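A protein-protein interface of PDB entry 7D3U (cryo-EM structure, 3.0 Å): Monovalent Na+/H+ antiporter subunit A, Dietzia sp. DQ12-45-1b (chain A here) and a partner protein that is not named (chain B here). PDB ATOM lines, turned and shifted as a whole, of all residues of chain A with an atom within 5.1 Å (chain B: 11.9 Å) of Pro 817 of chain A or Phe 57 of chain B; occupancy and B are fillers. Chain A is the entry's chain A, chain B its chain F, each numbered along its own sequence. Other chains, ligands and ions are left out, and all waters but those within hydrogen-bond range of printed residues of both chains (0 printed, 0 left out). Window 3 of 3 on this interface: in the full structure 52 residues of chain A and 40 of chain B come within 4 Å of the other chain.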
ATOM      1  N   PHE A 641      -6.807  33.232 -10.127  1.00  0.00           N
ATOM      2  CA  PHE A 641      -7.074  31.827 -10.402  1.00  0.00           C
ATOM      3  C   PHE A 641      -5.808  30.984 -10.329  1.00  0.00           C
ATOM      4  O   PHE A 641      -5.880  29.797  -9.997  1.00  0.00           O
ATOM      5  CB  PHE A 641      -7.734  31.671 -11.769  1.00  0.00           C
ATOM      6  CG  PHE A 641      -7.943  30.247 -12.177  1.00  0.00           C
ATOM      7  CD1 PHE A 641      -8.712  29.399 -11.403  1.00  0.00           C
ATOM      8  CD2 PHE A 641      -7.369  29.754 -13.332  1.00  0.00           C
ATOM      9  CE1 PHE A 641      -8.905  28.089 -11.775  1.00  0.00           C
ATOM     10  CE2 PHE A 641      -7.559  28.445 -13.707  1.00  0.00           C
ATOM     11  CZ  PHE A 641      -8.328  27.610 -12.928  1.00  0.00           C
ATOM     12  N   VAL A 646     -10.789  30.685  -6.836  1.00  0.00           N
ATOM     13  CA  VAL A 646     -11.717  30.561  -7.954  1.00  0.00           C
ATOM     14  C   VAL A 646     -12.857  31.563  -7.827  1.00  0.00           C
ATOM     15  O   VAL A 646     -13.216  32.240  -8.798  1.00  0.00           O
ATOM     16  CB  VAL A 646     -12.240  29.119  -8.054  1.00  0.00           C
ATOM     17  CG1 VAL A 646     -13.055  28.945  -9.318  1.00  0.00           C
ATOM     18  CG2 VAL A 646     -11.080  28.142  -8.029  1.00  0.00           C
ATOM     19  N   ASP A 647     -13.451  31.666  -6.635  1.00  0.00           N
ATOM     20  CA  ASP A 647     -14.532  32.626  -6.429  1.00  0.00           C
ATOM     21  C   ASP A 647     -14.038  34.054  -6.622  1.00  0.00           C
ATOM     22  O   ASP A 647     -14.734  34.892  -7.213  1.00  0.00           O
ATOM     23  CB  ASP A 647     -15.128  32.442  -5.034  1.00  0.00           C
ATOM     24  CG  ASP A 647     -16.501  33.072  -4.895  1.00  0.00           C
ATOM     25  OD1 ASP A 647     -16.939  33.769  -5.832  1.00  0.00           O
ATOM     26  OD2 ASP A 647     -17.144  32.869  -3.844  1.00  0.00           O
ATOM     27  N   LEU A 650     -13.685  34.658 -10.348  1.00  0.00           N
ATOM     28  CA  LEU A 650     -15.007  34.923 -10.904  1.00  0.00           C
ATOM     29  C   LEU A 650     -15.429  36.365 -10.657  1.00  0.00           C
ATOM     30  O   LEU A 650     -15.817  37.089 -11.587  1.00  0.00           O
ATOM     31  CB  LEU A 650     -16.019  33.959 -10.287  1.00  0.00           C
ATOM     32  CG  LEU A 650     -16.772  33.011 -11.207  1.00  0.00           C
ATOM     33  CD1 LEU A 650     -17.861  32.297 -10.433  1.00  0.00           C
ATOM     34  CD2 LEU A 650     -17.360  33.790 -12.355  1.00  0.00           C
ATOM     35  N   ASN A 728     -17.422  25.178   0.349  1.00  0.00           N
ATOM     36  CA  ASN A 728     -16.816  26.384  -0.211  1.00  0.00           C
ATOM     37  C   ASN A 728     -16.401  27.282   0.944  1.00  0.00           C
ATOM     38  O   ASN A 728     -17.191  28.092   1.432  1.00  0.00           O
ATOM     39  CB  ASN A 728     -17.794  27.088  -1.143  1.00  0.00           C
ATOM     40  CG  ASN A 728     -17.201  28.324  -1.798  1.00  0.00           C
ATOM     41  OD1 ASN A 728     -16.064  28.705  -1.529  1.00  0.00           O
ATOM     42  ND2 ASN A 728     -17.973  28.949  -2.677  1.00  0.00           N
ATOM     43  N   PHE A 809     -25.428  29.955 -10.031  1.00  0.00           N
ATOM     44  CA  PHE A 809     -24.444  30.298  -9.013  1.00  0.00           C
ATOM     45  C   PHE A 809     -25.107  30.628  -7.682  1.00  0.00           C
ATOM     46  O   PHE A 809     -24.497  30.437  -6.625  1.00  0.00           O
ATOM     47  CB  PHE A 809     -23.593  31.478  -9.478  1.00  0.00           C
ATOM     48  CG  PHE A 809     -22.679  31.160 -10.622  1.00  0.00           C
ATOM     49  CD1 PHE A 809     -22.278  29.861 -10.870  1.00  0.00           C
ATOM     50  CD2 PHE A 809     -22.216  32.166 -11.447  1.00  0.00           C
ATOM     51  CE1 PHE A 809     -21.435  29.573 -11.922  1.00  0.00           C
ATOM     52  CE2 PHE A 809     -21.374  31.882 -12.498  1.00  0.00           C
ATOM     53  CZ  PHE A 809     -20.983  30.584 -12.736  1.00  0.00           C
ATOM     54  N   ARG A 812     -25.753  27.136  -5.875  1.00  0.00           N
ATOM     55  CA  ARG A 812     -24.574  26.302  -5.700  1.00  0.00           C
ATOM     56  C   ARG A 812     -23.457  27.004  -4.943  1.00  0.00           C
ATOM     57  O   ARG A 812     -22.385  26.417  -4.765  1.00  0.00           O
ATOM     58  CB  ARG A 812     -24.050  25.838  -7.062  1.00  0.00           C
ATOM     59  CG  ARG A 812     -23.161  26.855  -7.756  1.00  0.00           C
ATOM     60  CD  ARG A 812     -22.953  26.500  -9.211  1.00  0.00           C
ATOM     61  NE  ARG A 812     -22.049  25.368  -9.376  1.00  0.00           N
ATOM     62  CZ  ARG A 812     -20.848  25.452  -9.935  1.00  0.00           C
ATOM     63  NH1 ARG A 812     -20.404  26.619 -10.379  1.00  0.00           N
ATOM     64  NH2 ARG A 812     -20.087  24.372 -10.045  1.00  0.00           N
ATOM     65  N   ASN A 815     -21.263  25.156  -2.076  1.00  0.00           N
ATOM     66  CA  ASN A 815     -20.376  24.031  -2.347  1.00  0.00           C
ATOM     67  C   ASN A 815     -19.671  24.177  -3.691  1.00  0.00           C
ATOM     68  O   ASN A 815     -19.172  23.188  -4.233  1.00  0.00           O
ATOM     69  CB  ASN A 815     -21.145  22.709  -2.299  1.00  0.00           C
ATOM     70  CG  ASN A 815     -21.919  22.532  -1.009  1.00  0.00           C
ATOM     71  OD1 ASN A 815     -22.866  23.268  -0.735  1.00  0.00           O
ATOM     72  ND2 ASN A 815     -21.519  21.552  -0.209  1.00  0.00           N
ATOM     73  N   ALA A 816     -19.615  25.389  -4.233  1.00  0.00           N
ATOM     74  CA  ALA A 816     -19.058  25.627  -5.555  1.00  0.00           C
ATOM     75  C   ALA A 816     -18.760  27.113  -5.684  1.00  0.00           C
ATOM     76  O   ALA A 816     -19.328  27.926  -4.947  1.00  0.00           O
ATOM     77  CB  ALA A 816     -20.027  25.167  -6.654  1.00  0.00           C
ATOM     78  N   PRO A 817     -17.870  27.499  -6.597  1.00  0.00           N
ATOM     79  CA  PRO A 817     -17.477  28.911  -6.688  1.00  0.00           C
ATOM     80  C   PRO A 817     -18.642  29.815  -7.068  1.00  0.00           C
ATOM     81  O   PRO A 817     -19.377  29.549  -8.019  1.00  0.00           O
ATOM     82  CB  PRO A 817     -16.393  28.906  -7.772  1.00  0.00           C
ATOM     83  CG  PRO A 817     -16.574  27.619  -8.499  1.00  0.00           C
ATOM     84  CD  PRO A 817     -17.044  26.653  -7.472  1.00  0.00           C
ATOM     85  N   GLY A 818     -18.804  30.890  -6.300  1.00  0.00           N
ATOM     86  CA  GLY A 818     -19.732  31.957  -6.621  1.00  0.00           C
ATOM     87  C   GLY A 818     -21.036  31.876  -5.859  1.00  0.00           C
ATOM     88  O   GLY A 818     -21.926  31.121  -6.254  1.00  0.00           O
ATOM     89  N   GLY A 819     -21.173  32.636  -4.772  1.00  0.00           N
ATOM     90  CA  GLY A 819     -22.388  32.529  -3.987  1.00  0.00           C
ATOM     91  C   GLY A 819     -23.485  33.540  -4.253  1.00  0.00           C
ATOM     92  O   GLY A 819     -24.582  33.156  -4.666  1.00  0.00           O
ATOM     93  N   ILE B  43      -8.819  33.933 -21.932  1.00  0.00           N
ATOM     94  CA  ILE B  43      -9.651  32.762 -21.658  1.00  0.00           C
ATOM     95  C   ILE B  43      -8.870  31.481 -21.936  1.00  0.00           C
ATOM     96  O   ILE B  43      -8.929  30.511 -21.163  1.00  0.00           O
ATOM     97  CB  ILE B  43     -10.951  32.820 -22.478  1.00  0.00           C
ATOM     98  CG1 ILE B  43     -11.695  34.123 -22.203  1.00  0.00           C
ATOM     99  CG2 ILE B  43     -11.836  31.638 -22.150  1.00  0.00           C
ATOM    100  CD1 ILE B  43     -12.964  34.268 -22.999  1.00  0.00           C
ATOM    101  N   LEU B  45      -5.663  31.136 -21.726  1.00  0.00           N
ATOM    102  CA  LEU B  45      -4.686  30.997 -20.654  1.00  0.00           C
ATOM    103  C   LEU B  45      -5.341  30.512 -19.371  1.00  0.00           C
ATOM    104  O   LEU B  45      -4.744  29.734 -18.625  1.00  0.00           O
ATOM    105  CB  LEU B  45      -3.966  32.321 -20.419  1.00  0.00           C
ATOM    106  CG  LEU B  45      -2.645  32.477 -21.165  1.00  0.00           C
ATOM    107  CD1 LEU B  45      -1.811  33.548 -20.511  1.00  0.00           C
ATOM    108  CD2 LEU B  45      -1.894  31.161 -21.193  1.00  0.00           C
ATOM    109  N   LEU B  46      -6.564  30.967 -19.091  1.00  0.00           N
ATOM    110  CA  LEU B  46      -7.308  30.440 -17.952  1.00  0.00           C
ATOM    111  C   LEU B  46      -7.463  28.932 -18.064  1.00  0.00           C
ATOM    112  O   LEU B  46      -7.185  28.193 -17.112  1.00  0.00           O
ATOM    113  CB  LEU B  46      -8.677  31.112 -17.859  1.00  0.00           C
ATOM    114  CG  LEU B  46      -8.757  32.460 -17.146  1.00  0.00           C
ATOM    115  CD1 LEU B  46     -10.198  32.929 -17.063  1.00  0.00           C
ATOM    116  CD2 LEU B  46      -8.154  32.356 -15.763  1.00  0.00           C
ATOM    117  N   ALA B  47      -7.895  28.458 -19.233  1.00  0.00           N
ATOM    118  CA  ALA B  47      -8.076  27.021 -19.426  1.00  0.00           C
ATOM    119  C   ALA B  47      -6.762  26.266 -19.251  1.00  0.00           C
ATOM    120  O   ALA B  47      -6.689  25.272 -18.515  1.00  0.00           O
ATOM    121  CB  ALA B  47      -8.667  26.751 -20.808  1.00  0.00           C
ATOM    122  N   LEU B  48      -5.707  26.728 -19.920  1.00  0.00           N
ATOM    123  CA  LEU B  48      -4.437  26.010 -19.880  1.00  0.00           C
ATOM    124  C   LEU B  48      -3.823  26.030 -18.485  1.00  0.00           C
ATOM    125  O   LEU B  48      -3.226  25.038 -18.048  1.00  0.00           O
ATOM    126  CB  LEU B  48      -3.478  26.601 -20.906  1.00  0.00           C
ATOM    127  CG  LEU B  48      -3.907  26.413 -22.360  1.00  0.00           C
ATOM    128  CD1 LEU B  48      -2.898  27.035 -23.303  1.00  0.00           C
ATOM    129  CD2 LEU B  48      -4.087  24.939 -22.664  1.00  0.00           C
ATOM    130  N   VAL B  49      -3.957  27.146 -17.765  1.00  0.00           N
ATOM    131  CA  VAL B  49      -3.449  27.217 -16.403  1.00  0.00           C
ATOM    132  C   VAL B  49      -4.233  26.282 -15.496  1.00  0.00           C
ATOM    133  O   VAL B  49      -3.649  25.525 -14.713  1.00  0.00           O
ATOM    134  CB  VAL B  49      -3.485  28.670 -15.898  1.00  0.00           C
ATOM    135  CG1 VAL B  49      -3.615  28.707 -14.389  1.00  0.00           C
ATOM    136  CG2 VAL B  49      -2.241  29.411 -16.348  1.00  0.00           C
ATOM    137  N   GLY B  50      -5.566  26.301 -15.597  1.00  0.00           N
ATOM    138  CA  GLY B  50      -6.368  25.342 -14.865  1.00  0.00           C
ATOM    139  C   GLY B  50      -6.007  23.908 -15.171  1.00  0.00           C
ATOM    140  O   GLY B  50      -6.215  23.030 -14.328  1.00  0.00           O
ATOM    141  N   VAL B  51      -5.475  23.648 -16.364  1.00  0.00           N
ATOM    142  CA  VAL B  51      -4.913  22.330 -16.640  1.00  0.00           C
ATOM    143  C   VAL B  51      -3.621  22.130 -15.856  1.00  0.00           C
ATOM    144  O   VAL B  51      -3.422  21.092 -15.214  1.00  0.00           O
ATOM    145  CB  VAL B  51      -4.686  22.138 -18.148  1.00  0.00           C
ATOM    146  CG1 VAL B  51      -3.864  20.892 -18.387  1.00  0.00           C
ATOM    147  CG2 VAL B  51      -6.004  22.039 -18.863  1.00  0.00           C
ATOM    148  N   ARG B  52      -2.723  23.116 -15.897  1.00  0.00           N
ATOM    149  CA  ARG B  52      -1.439  22.998 -15.211  1.00  0.00           C
ATOM    150  C   ARG B  52      -1.623  22.815 -13.710  1.00  0.00           C
ATOM    151  O   ARG B  52      -1.245  21.776 -13.159  1.00  0.00           O
ATOM    152  CB  ARG B  52      -0.557  24.215 -15.487  1.00  0.00           C
ATOM    153  CG  ARG B  52       0.837  24.097 -14.900  1.00  0.00           C
ATOM    154  CD  ARG B  52       1.708  25.278 -15.277  1.00  0.00           C
ATOM    155  NE  ARG B  52       3.039  25.173 -14.693  1.00  0.00           N
ATOM    156  CZ  ARG B  52       4.035  24.466 -15.220  1.00  0.00           C
ATOM    157  NH1 ARG B  52       5.214  24.432 -14.615  1.00  0.00           N
ATOM    158  NH2 ARG B  52       3.851  23.793 -16.344  1.00  0.00           N
ATOM    159  N   VAL B  53      -2.200  23.809 -13.039  1.00  0.00           N
ATOM    160  CA  VAL B  53      -2.609  23.643 -11.645  1.00  0.00           C
ATOM    161  C   VAL B  53      -3.956  22.924 -11.667  1.00  0.00           C
ATOM    162  O   VAL B  53      -5.013  23.544 -11.810  1.00  0.00           O
ATOM    163  CB  VAL B  53      -2.659  24.973 -10.885  1.00  0.00           C
ATOM    164  CG1 VAL B  53      -1.258  25.511 -10.697  1.00  0.00           C
ATOM    165  CG2 VAL B  53      -3.479  26.018 -11.624  1.00  0.00           C
ATOM    166  N   ASP B  54      -3.912  21.598 -11.546  1.00  0.00           N
ATOM    167  CA  ASP B  54      -5.077  20.762 -11.811  1.00  0.00           C
ATOM    168  C   ASP B  54      -6.238  21.191 -10.928  1.00  0.00           C
ATOM    169  O   ASP B  54      -6.202  21.013  -9.706  1.00  0.00           O
ATOM    170  CB  ASP B  54      -4.733  19.294 -11.573  1.00  0.00           C
ATOM    171  CG  ASP B  54      -5.611  18.353 -12.371  1.00  0.00           C
ATOM    172  OD1 ASP B  54      -6.849  18.515 -12.334  1.00  0.00           O
ATOM    173  OD2 ASP B  54      -5.062  17.452 -13.040  1.00  0.00           O
ATOM    174  N   SER B  55      -7.272  21.756 -11.553  1.00  0.00           N
ATOM    175  CA  SER B  55      -8.389  22.345 -10.845  1.00  0.00           C
ATOM    176  C   SER B  55      -9.681  21.900 -11.516  1.00  0.00           C
ATOM    177  O   SER B  55      -9.777  21.935 -12.755  1.00  0.00           O
ATOM    178  CB  SER B  55      -8.292  23.871 -10.832  1.00  0.00           C
ATOM    179  OG  SER B  55      -8.959  24.418  -9.709  1.00  0.00           O
ATOM    180  N   PRO B  56     -10.683  21.466 -10.745  1.00  0.00           N
ATOM    181  CA  PRO B  56     -11.970  21.113 -11.356  1.00  0.00           C
ATOM    182  C   PRO B  56     -12.834  22.314 -11.686  1.00  0.00           C
ATOM    183  O   PRO B  56     -13.675  22.220 -12.591  1.00  0.00           O
ATOM    184  CB  PRO B  56     -12.642  20.236 -10.286  1.00  0.00           C
ATOM    185  CG  PRO B  56     -11.573  19.958  -9.254  1.00  0.00           C
ATOM    186  CD  PRO B  56     -10.639  21.115  -9.320  1.00  0.00           C
ATOM    187  N   PHE B  57     -12.660  23.428 -10.985  1.00  0.00           N
ATOM    188  CA  PHE B  57     -13.511  24.608 -11.134  1.00  0.00           C
ATOM    189  C   PHE B  57     -12.918  25.606 -12.117  1.00  0.00           C
ATOM    190  O   PHE B  57     -12.744  26.782 -11.806  1.00  0.00           O
ATOM    191  CB  PHE B  57     -13.737  25.251  -9.772  1.00  0.00           C
ATOM    192  CG  PHE B  57     -13.815  24.260  -8.652  1.00  0.00           C
ATOM    193  CD1 PHE B  57     -15.011  23.635  -8.347  1.00  0.00           C
ATOM    194  CD2 PHE B  57     -12.688  23.938  -7.915  1.00  0.00           C
ATOM    195  CE1 PHE B  57     -15.084  22.716  -7.322  1.00  0.00           C
ATOM    196  CE2 PHE B  57     -12.755  23.020  -6.893  1.00  0.00           C
ATOM    197  CZ  PHE B  57     -13.955  22.407  -6.594  1.00  0.00           C
ATOM    198  N   VAL B  58     -12.595  25.147 -13.321  1.00  0.00           N
ATOM    199  CA  VAL B  58     -12.060  26.030 -14.350  1.00  0.00           C
ATOM    200  C   VAL B  58     -13.162  26.567 -15.246  1.00  0.00           C
ATOM    201  O   VAL B  58     -13.277  27.777 -15.458  1.00  0.00           O
ATOM    202  CB  VAL B  58     -10.987  25.292 -15.174  1.00  0.00           C
ATOM    203  CG1 VAL B  58     -10.377  26.227 -16.195  1.00  0.00           C
ATOM    204  CG2 VAL B  58      -9.920  24.735 -14.264  1.00  0.00           C
ATOM    205  N   TYR B  59     -14.002  25.674 -15.767  1.00  0.00           N
ATOM    206  CA  TYR B  59     -14.879  26.039 -16.868  1.00  0.00           C
ATOM    207  C   TYR B  59     -16.021  26.942 -16.438  1.00  0.00           C
ATOM    208  O   TYR B  59     -16.577  27.649 -17.286  1.00  0.00           O
ATOM    209  CB  TYR B  59     -15.380  24.772 -17.548  1.00  0.00           C
ATOM    210  CG  TYR B  59     -14.222  24.060 -18.181  1.00  0.00           C
ATOM    211  CD1 TYR B  59     -13.537  24.640 -19.237  1.00  0.00           C
ATOM    212  CD2 TYR B  59     -13.763  22.853 -17.683  1.00  0.00           C
ATOM    213  CE1 TYR B  59     -12.460  24.020 -19.805  1.00  0.00           C
ATOM    214  CE2 TYR B  59     -12.681  22.223 -18.248  1.00  0.00           C
ATOM    215  CZ  TYR B  59     -12.035  22.815 -19.308  1.00  0.00           C
ATOM    216  OH  TYR B  59     -10.953  22.205 -19.881  1.00  0.00           O
ATOM    217  N   ASP B  60     -16.376  26.944 -15.152  1.00  0.00           N
ATOM    218  CA  ASP B  60     -17.206  28.018 -14.622  1.00  0.00           C
ATOM    219  C   ASP B  60     -16.676  29.362 -15.098  1.00  0.00           C
ATOM    220  O   ASP B  60     -17.369  30.114 -15.793  1.00  0.00           O
ATOM    221  CB  ASP B  60     -17.233  27.956 -13.094  1.00  0.00           C
ATOM    222  CG  ASP B  60     -17.542  26.570 -12.574  1.00  0.00           C
ATOM    223  OD1 ASP B  60     -18.126  25.769 -13.330  1.00  0.00           O
ATOM    224  OD2 ASP B  60     -17.200  26.277 -11.411  1.00  0.00           O
ATOM    225  N   LEU B  61     -15.414  29.649 -14.771  1.00  0.00           N
ATOM    226  CA  LEU B  61     -14.755  30.847 -15.278  1.00  0.00           C
ATOM    227  C   LEU B  61     -14.830  30.908 -16.798  1.00  0.00           C
ATOM    228  O   LEU B  61     -15.148  31.953 -17.376  1.00  0.00           O
ATOM    229  CB  LEU B  61     -13.300  30.873 -14.814  1.00  0.00           C
ATOM    230  CG  LEU B  61     -13.073  30.719 -13.314  1.00  0.00           C
ATOM    231  CD1 LEU B  61     -11.603  30.514 -13.028  1.00  0.00           C
ATOM    232  CD2 LEU B  61     -13.593  31.934 -12.580  1.00  0.00           C
ATOM    233  N   VAL B  62     -14.560  29.782 -17.462  1.00  0.00           N
ATOM    234  CA  VAL B  62     -14.608  29.768 -18.918  1.00  0.00           C
ATOM    235  C   VAL B  62     -16.027  30.020 -19.402  1.00  0.00           C
ATOM    236  O   VAL B  62     -16.233  30.680 -20.428  1.00  0.00           O
ATOM    237  CB  VAL B  62     -14.042  28.443 -19.456  1.00  0.00           C
ATOM    238  CG1 VAL B  62     -14.410  28.252 -20.915  1.00  0.00           C
ATOM    239  CG2 VAL B  62     -12.536  28.406 -19.277  1.00  0.00           C
ATOM    240  N   LEU B  63     -17.029  29.533 -18.669  1.00  0.00           N
ATOM    241  CA  LEU B  63     -18.405  29.837 -19.035  1.00  0.00           C
ATOM    242  C   LEU B  63     -18.747  31.296 -18.771  1.00  0.00           C
ATOM    243  O   LEU B  63     -19.663  31.833 -19.403  1.00  0.00           O
ATOM    244  CB  LEU B  63     -19.366  28.920 -18.279  1.00  0.00           C
ATOM    245  CG  LEU B  63     -20.847  29.030 -18.632  1.00  0.00           C
ATOM    246  CD1 LEU B  63     -21.034  28.931 -20.133  1.00  0.00           C
ATOM    247  CD2 LEU B  63     -21.639  27.951 -17.920  1.00  0.00           C
ATOM    248  N   VAL B  64     -18.024  31.949 -17.867  1.00  0.00           N
ATOM    249  CA  VAL B  64     -18.310  33.336 -17.518  1.00  0.00           C
ATOM    250  C   VAL B  64     -17.443  34.301 -18.315  1.00  0.00           C
ATOM    251  O   VAL B  64     -17.925  35.342 -18.768  1.00  0.00           O
ATOM    252  CB  VAL B  64     -18.130  33.533 -16.002  1.00  0.00           C
ATOM    253  CG1 VAL B  64     -18.041  35.007 -15.664  1.00  0.00           C
ATOM    254  CG2 VAL B  64     -19.272  32.875 -15.256  1.00  0.00           C
ATOM    255  N   ALA B  65     -16.162  33.970 -18.503  1.00  0.00           N
ATOM    256  CA  ALA B  65     -15.267  34.862 -19.232  1.00  0.00           C
ATOM    257  C   ALA B  65     -15.758  35.119 -20.650  1.00  0.00           C
ATOM    258  O   ALA B  65     -15.547  36.211 -21.189  1.00  0.00           O
ATOM    259  CB  ALA B  65     -13.853  34.284 -19.256  1.00  0.00           C
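O of Phe 809 of chain A lies close to O of Gly 818 of chain A (2.7 Å). The backbone carbonyl oxygen of Gly 50 of chain B is in hydrogen-bond range of the backbone NH of Ser 55 of chain B (3.2 Å).
Leu 46 of chain B touches Phe 641 of chain A. CE2 of Phe 641 of chain A touches N of Gly 50 of chain B, at 3.5 Å. Phe 641 of chain A touches Val 58 of chain B (CZ to CG2, 3.5 Å). Leu 61 of chain B touches Phe 641 of chain A. Val 646 of chain A touches Phe 57 of chain B (CG1 to O, 3.3 Å). Val 646 of chain A touches Leu 61 of chain B. N of Leu 650 of chain A touches CD2 of Leu 61 of chain B (3.5 Å). Val 64 of chain B touches Leu 650 of chain A (CG1 to CD2, 3.6 Å). CE2 of Phe 809 of chain A touches CG2 of Val 64 of chain B, at 3.6 Å. Pro 817 of chain A touches Phe 57 of chain B (CD to CD1, 3.7 Å).
Of chain A, only Val 646 and Pro 817 come within 4 Å of Phe 57 of chain B. Printed residues of chain B within 4 Å of Val 646 of chain A: Phe 57 (3.3 Å) and Leu 61 (3.8 Å). Arg 812 of chain A touches one residue of chain B. No residue of chain B comes within 4 Å of Ala 816 of chain A. No residue of chain B comes within 4 Å of Gly 818 of chain A. No residue of chain B comes within 4 Å of Gly 819 of chain A. Of the printed residues of chain B, Leu 650 of chain A touches Leu 61 and Val 64. Printed residues of chain A within 4 Å of Val 58 of chain B: Phe 641 (3.5 Å). Printed residues of chain A within 4 Å of Leu 61 of chain B: Phe 641 (3.5 Å), Val 646 (3.8 Å) and Leu 650 (3.5 Å). Leu 63 of chain B touches none of the printed residues of chain A. The nearest residue of chain B that does not touch Pro 817 of chain A is Leu 61 of chain B (6.3 Å). The nearest residue of chain A that does not touch Phe 57 of chain B is Phe 641 of chain A (4.1 Å).
Of the 22 printed residues of chain B, 7 touch a printed residue of chain A. Hydrophobic or aromatic side chains of chain B within 4 Å of the printed part of chain A: Leu 46, Phe 57, Val 58, Leu 61 and Val 64. Hydrophobic or aromatic side chains of chain A that line the printed part of chain B: Phe 641, Val 646, Leu 650, Phe 809 and Pro 817. Among the printed residues, Asp or Glu carboxylates within 4 Å of a Lys or Arg side-chain nitrogen of the other chain: Arg 812 of chain A with Asp 60 of chain B (3.4 Å).
NH1 of Arg 812 of chain A is in salt-bridge range of OD2 of Asp 60 of chain B, at 3.4 Å.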
